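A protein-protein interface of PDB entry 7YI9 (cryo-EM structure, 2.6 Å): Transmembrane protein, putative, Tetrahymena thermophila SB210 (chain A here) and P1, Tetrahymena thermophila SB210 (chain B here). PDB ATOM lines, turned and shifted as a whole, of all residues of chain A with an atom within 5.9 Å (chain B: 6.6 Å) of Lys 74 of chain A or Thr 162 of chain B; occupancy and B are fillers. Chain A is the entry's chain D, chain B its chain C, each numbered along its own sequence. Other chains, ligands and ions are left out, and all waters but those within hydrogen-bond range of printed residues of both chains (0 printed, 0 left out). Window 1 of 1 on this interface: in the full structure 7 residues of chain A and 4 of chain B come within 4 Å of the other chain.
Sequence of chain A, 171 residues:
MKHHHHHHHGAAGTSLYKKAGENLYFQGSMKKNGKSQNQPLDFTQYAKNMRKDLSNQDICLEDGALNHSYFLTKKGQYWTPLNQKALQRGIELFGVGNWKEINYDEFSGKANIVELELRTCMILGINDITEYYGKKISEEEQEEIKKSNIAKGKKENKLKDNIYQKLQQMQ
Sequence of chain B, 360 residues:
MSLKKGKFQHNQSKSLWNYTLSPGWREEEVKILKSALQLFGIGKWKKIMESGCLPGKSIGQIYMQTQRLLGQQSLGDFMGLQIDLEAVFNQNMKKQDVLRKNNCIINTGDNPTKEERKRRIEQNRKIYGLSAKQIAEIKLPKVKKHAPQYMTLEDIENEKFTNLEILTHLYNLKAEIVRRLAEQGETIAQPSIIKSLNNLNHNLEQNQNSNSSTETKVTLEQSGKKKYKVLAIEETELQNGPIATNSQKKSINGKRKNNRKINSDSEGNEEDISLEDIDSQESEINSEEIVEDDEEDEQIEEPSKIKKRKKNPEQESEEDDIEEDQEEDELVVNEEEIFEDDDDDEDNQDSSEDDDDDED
The side-chain hydroxyl (OG1) of Thr 162 of chain B lies close to the side-chain hydroxyl (OG1) of Thr 73 of chain A, 3.5 Å away.
OG1 of Thr 162 of chain B sits at hydrogen-bond distance from N of Lys 74 of chain A (3.5 Å).
OE2 of Glu 165 of chain B is in salt-bridge range of NZ of Lys 74 of chain A (2.9 Å).
O of Leu 72 of chain A touches OG1 of Thr 162 of chain B (3.5 Å).
CD2 of Leu 164 of chain B touches NE2 of Gln 77 of chain A, 3.4 Å away.
Gln 77 of chain A touches Glu 165 of chain B.
Of the printed residues of chain B, Leu 72 of chain A touches Thr 162 (3.5 Å).
Of the printed residues of chain B, Thr 73 of chain A touches Thr 162.
Printed residues of chain A within 4 Å of Thr 162 of chain B: Leu 72 (3.5 Å), Thr 73 (3.2 Å) and Lys 74 (3.5 Å).
The nearest printed residue of chain A that does not touch Leu 164 of chain B is Thr 73 of chain A (5.0 Å).
Of the 8 printed residues of chain A, 4 touch a printed residue of chain B.
Among the printed residues, 6 pairs touch across the chains.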
ATOM      1  N   TYR A  70      12.054  -0.643   3.866  1.00  0.00           N
ATOM      2  CA  TYR A  70      12.536  -1.948   4.305  1.00  0.00           C
ATOM      3  C   TYR A  70      13.550  -1.815   5.433  1.00  0.00           C
ATOM      4  O   TYR A  70      13.517  -2.585   6.401  1.00  0.00           O
ATOM      5  CB  TYR A  70      13.144  -2.703   3.122  1.00  0.00           C
ATOM      6  CG  TYR A  70      13.535  -4.127   3.438  1.00  0.00           C
ATOM      7  CD1 TYR A  70      12.573  -5.119   3.569  1.00  0.00           C
ATOM      8  CD2 TYR A  70      14.867  -4.481   3.610  1.00  0.00           C
ATOM      9  CE1 TYR A  70      12.926  -6.421   3.861  1.00  0.00           C
ATOM     10  CE2 TYR A  70      15.228  -5.779   3.903  1.00  0.00           C
ATOM     11  CZ  TYR A  70      14.254  -6.745   4.026  1.00  0.00           C
ATOM     12  OH  TYR A  70      14.608  -8.042   4.316  1.00  0.00           O
ATOM     13  N   LEU A  72      13.845   0.763   7.472  1.00  0.00           N
ATOM     14  CA  LEU A  72      13.283   1.465   8.615  1.00  0.00           C
ATOM     15  C   LEU A  72      12.492   0.543   9.525  1.00  0.00           C
ATOM     16  O   LEU A  72      11.884   1.015  10.490  1.00  0.00           O
ATOM     17  CB  LEU A  72      12.391   2.619   8.150  1.00  0.00           C
ATOM     18  CG  LEU A  72      13.122   3.901   7.744  1.00  0.00           C
ATOM     19  CD1 LEU A  72      12.265   4.751   6.821  1.00  0.00           C
ATOM     20  CD2 LEU A  72      13.539   4.686   8.974  1.00  0.00           C
ATOM     21  N   THR A  73      12.483  -0.755   9.235  1.00  0.00           N
ATOM     22  CA  THR A  73      11.791  -1.740  10.049  1.00  0.00           C
ATOM     23  C   THR A  73      12.700  -2.943  10.249  1.00  0.00           C
ATOM     24  O   THR A  73      13.626  -3.185   9.472  1.00  0.00           O
ATOM     25  CB  THR A  73      10.462  -2.171   9.413  1.00  0.00           C
ATOM     26  OG1 THR A  73       9.853  -3.193  10.211  1.00  0.00           O
ATOM     27  CG2 THR A  73      10.684  -2.690   8.003  1.00  0.00           C
ATOM     28  N   LYS A  74      12.430  -3.688  11.318  1.00  0.00           N
ATOM     29  CA  LYS A  74      13.200  -4.885  11.617  1.00  0.00           C
ATOM     30  C   LYS A  74      12.987  -5.936  10.533  1.00  0.00           C
ATOM     31  O   LYS A  74      11.935  -5.992   9.891  1.00  0.00           O
ATOM     32  CB  LYS A  74      12.800  -5.444  12.982  1.00  0.00           C
ATOM     33  CG  LYS A  74      13.838  -6.351  13.611  1.00  0.00           C
ATOM     34  CD  LYS A  74      13.342  -6.934  14.921  1.00  0.00           C
ATOM     35  CE  LYS A  74      12.429  -8.122  14.675  1.00  0.00           C
ATOM     36  NZ  LYS A  74      12.169  -8.896  15.919  1.00  0.00           N
ATOM     37  N   LYS A  75      14.005  -6.769  10.324  1.00  0.00           N
ATOM     38  CA  LYS A  75      13.941  -7.767   9.265  1.00  0.00           C
ATOM     39  C   LYS A  75      12.827  -8.772   9.530  1.00  0.00           C
ATOM     40  O   LYS A  75      12.602  -9.193  10.667  1.00  0.00           O
ATOM     41  CB  LYS A  75      15.276  -8.500   9.135  1.00  0.00           C
ATOM     42  CG  LYS A  75      15.287  -9.514   8.009  1.00  0.00           C
ATOM     43  CD  LYS A  75      16.467 -10.452   8.097  1.00  0.00           C
ATOM     44  CE  LYS A  75      16.470 -11.421   6.932  1.00  0.00           C
ATOM     45  NZ  LYS A  75      15.287 -12.320   6.958  1.00  0.00           N
ATOM     46  N   GLY A  76      12.131  -9.160   8.463  1.00  0.00           N
ATOM     47  CA  GLY A  76      11.042 -10.106   8.568  1.00  0.00           C
ATOM     48  C   GLY A  76       9.714  -9.512   8.970  1.00  0.00           C
ATOM     49  O   GLY A  76       8.753 -10.263   9.174  1.00  0.00           O
ATOM     50  N   GLN A  77       9.622  -8.186   9.090  1.00  0.00           N
ATOM     51  CA  GLN A  77       8.376  -7.524   9.449  1.00  0.00           C
ATOM     52  C   GLN A  77       7.974  -6.459   8.439  1.00  0.00           C
ATOM     53  O   GLN A  77       7.091  -5.647   8.733  1.00  0.00           O
ATOM     54  CB  GLN A  77       8.480  -6.898  10.845  1.00  0.00           C
ATOM     55  CG  GLN A  77       9.047  -7.825  11.902  1.00  0.00           C
ATOM     56  CD  GLN A  77       8.353  -7.674  13.239  1.00  0.00           C
ATOM     57  OE1 GLN A  77       8.957  -7.237  14.218  1.00  0.00           O
ATOM     58  NE2 GLN A  77       7.077  -8.035  13.287  1.00  0.00           N
ATOM     59  N   TYR A  78       8.595  -6.437   7.263  1.00  0.00           N
ATOM     60  CA  TYR A  78       8.287  -5.429   6.260  1.00  0.00           C
ATOM     61  C   TYR A  78       6.977  -5.765   5.559  1.00  0.00           C
ATOM     62  O   TYR A  78       6.766  -6.902   5.127  1.00  0.00           O
ATOM     63  CB  TYR A  78       9.424  -5.328   5.246  1.00  0.00           C
ATOM     64  CG  TYR A  78       9.069  -4.558   3.998  1.00  0.00           C
ATOM     65  CD1 TYR A  78       8.634  -3.241   4.070  1.00  0.00           C
ATOM     66  CD2 TYR A  78       9.175  -5.144   2.746  1.00  0.00           C
ATOM     67  CE1 TYR A  78       8.311  -2.535   2.930  1.00  0.00           C
ATOM     68  CE2 TYR A  78       8.855  -4.445   1.602  1.00  0.00           C
ATOM     69  CZ  TYR A  78       8.424  -3.143   1.698  1.00  0.00           C
ATOM     70  OH  TYR A  78       8.105  -2.448   0.556  1.00  0.00           O
ATOM     71  N   LYS B 160      14.272  -0.486  22.856  1.00  0.00           N
ATOM     72  CA  LYS B 160      13.946   0.204  21.614  1.00  0.00           C
ATOM     73  C   LYS B 160      13.716  -0.836  20.522  1.00  0.00           C
ATOM     74  O   LYS B 160      14.556  -1.714  20.293  1.00  0.00           O
ATOM     75  CB  LYS B 160      15.044   1.200  21.241  1.00  0.00           C
ATOM     76  CG  LYS B 160      16.401   0.598  20.918  1.00  0.00           C
ATOM     77  CD  LYS B 160      17.396   1.682  20.543  1.00  0.00           C
ATOM     78  CE  LYS B 160      17.826   2.481  21.759  1.00  0.00           C
ATOM     79  NZ  LYS B 160      18.898   3.459  21.430  1.00  0.00           N
ATOM     80  N   PHE B 161      12.562  -0.758  19.872  1.00  0.00           N
ATOM     81  CA  PHE B 161      12.171  -1.682  18.821  1.00  0.00           C
ATOM     82  C   PHE B 161      11.970  -0.929  17.513  1.00  0.00           C
ATOM     83  O   PHE B 161      12.226   0.274  17.408  1.00  0.00           O
ATOM     84  CB  PHE B 161      10.882  -2.421  19.197  1.00  0.00           C
ATOM     85  CG  PHE B 161      10.964  -3.174  20.495  1.00  0.00           C
ATOM     86  CD1 PHE B 161      11.971  -4.096  20.716  1.00  0.00           C
ATOM     87  CD2 PHE B 161      10.019  -2.972  21.484  1.00  0.00           C
ATOM     88  CE1 PHE B 161      12.038  -4.793  21.902  1.00  0.00           C
ATOM     89  CE2 PHE B 161      10.082  -3.665  22.672  1.00  0.00           C
ATOM     90  CZ  PHE B 161      11.092  -4.577  22.882  1.00  0.00           C
ATOM     91  N   THR B 162      11.510  -1.663  16.506  1.00  0.00           N
ATOM     92  CA  THR B 162      10.973  -1.016  15.323  1.00  0.00           C
ATOM     93  C   THR B 162       9.541  -0.569  15.597  1.00  0.00           C
ATOM     94  O   THR B 162       8.942  -0.909  16.620  1.00  0.00           O
ATOM     95  CB  THR B 162      11.013  -1.950  14.114  1.00  0.00           C
ATOM     96  OG1 THR B 162      10.646  -1.217  12.940  1.00  0.00           O
ATOM     97  CG2 THR B 162      10.044  -3.103  14.295  1.00  0.00           C
ATOM     98  N   ASN B 163       8.992   0.206  14.661  1.00  0.00           N
ATOM     99  CA  ASN B 163       7.665   0.776  14.867  1.00  0.00           C
ATOM    100  C   ASN B 163       6.593  -0.298  15.009  1.00  0.00           C
ATOM    101  O   ASN B 163       5.641  -0.121  15.776  1.00  0.00           O
ATOM    102  CB  ASN B 163       7.311   1.716  13.719  1.00  0.00           C
ATOM    103  CG  ASN B 163       6.124   2.590  14.039  1.00  0.00           C
ATOM    104  OD1 ASN B 163       6.025   3.148  15.131  1.00  0.00           O
ATOM    105  ND2 ASN B 163       5.207   2.704  13.089  1.00  0.00           N
ATOM    106  N   LEU B 164       6.708  -1.399  14.270  1.00  0.00           N
ATOM    107  CA  LEU B 164       5.688  -2.437  14.357  1.00  0.00           C
ATOM    108  C   LEU B 164       5.823  -3.268  15.627  1.00  0.00           C
ATOM    109  O   LEU B 164       4.809  -3.641  16.227  1.00  0.00           O
ATOM    110  CB  LEU B 164       5.754  -3.337  13.121  1.00  0.00           C
ATOM    111  CG  LEU B 164       4.957  -4.640  13.162  1.00  0.00           C
ATOM    112  CD1 LEU B 164       3.467  -4.353  13.231  1.00  0.00           C
ATOM    113  CD2 LEU B 164       5.280  -5.486  11.950  1.00  0.00           C
ATOM    114  N   GLU B 165       7.052  -3.547  16.059  1.00  0.00           N
ATOM    115  CA  GLU B 165       7.317  -4.452  17.171  1.00  0.00           C
ATOM    116  C   GLU B 165       7.007  -3.850  18.538  1.00  0.00           C
ATOM    117  O   GLU B 165       6.913  -4.604  19.513  1.00  0.00           O
ATOM    118  CB  GLU B 165       8.782  -4.894  17.127  1.00  0.00           C
ATOM    119  CG  GLU B 165       9.118  -6.104  17.978  1.00  0.00           C
ATOM    120  CD  GLU B 165      10.589  -6.456  17.915  1.00  0.00           C
ATOM    121  OE1 GLU B 165      11.398  -5.567  17.575  1.00  0.00           O
ATOM    122  OE2 GLU B 165      10.939  -7.618  18.208  1.00  0.00           O
ATOM    123  N   ILE B 166       6.821  -2.529  18.632  1.00  0.00           N
ATOM    124  CA  ILE B 166       6.689  -1.868  19.933  1.00  0.00           C
ATOM    125  C   ILE B 166       5.548  -2.457  20.749  1.00  0.00           C
ATOM    126  O   ILE B 166       5.534  -2.343  21.980  1.00  0.00           O
ATOM    127  CB  ILE B 166       6.516  -0.348  19.749  1.00  0.00           C
ATOM    128  CG1 ILE B 166       5.350  -0.045  18.805  1.00  0.00           C
ATOM    129  CG2 ILE B 166       7.805   0.280  19.249  1.00  0.00           C
ATOM    130  CD1 ILE B 166       5.104   1.437  18.586  1.00  0.00           C
ATOM    131  N   LEU B 167       4.575  -3.081  20.094  1.00  0.00           N
ATOM    132  CA  LEU B 167       3.533  -3.829  20.793  1.00  0.00           C
ATOM    133  C   LEU B 167       3.948  -5.290  20.966  1.00  0.00           C
ATOM    134  O   LEU B 167       3.219  -6.209  20.603  1.00  0.00           O
ATOM    135  CB  LEU B 167       2.212  -3.724  20.037  1.00  0.00           C
ATOM    136  CG  LEU B 167       1.362  -2.449  20.073  1.00  0.00           C
ATOM    137  CD1 LEU B 167       1.987  -1.332  19.251  1.00  0.00           C
ATOM    138  CD2 LEU B 167      -0.053  -2.726  19.591  1.00  0.00           C
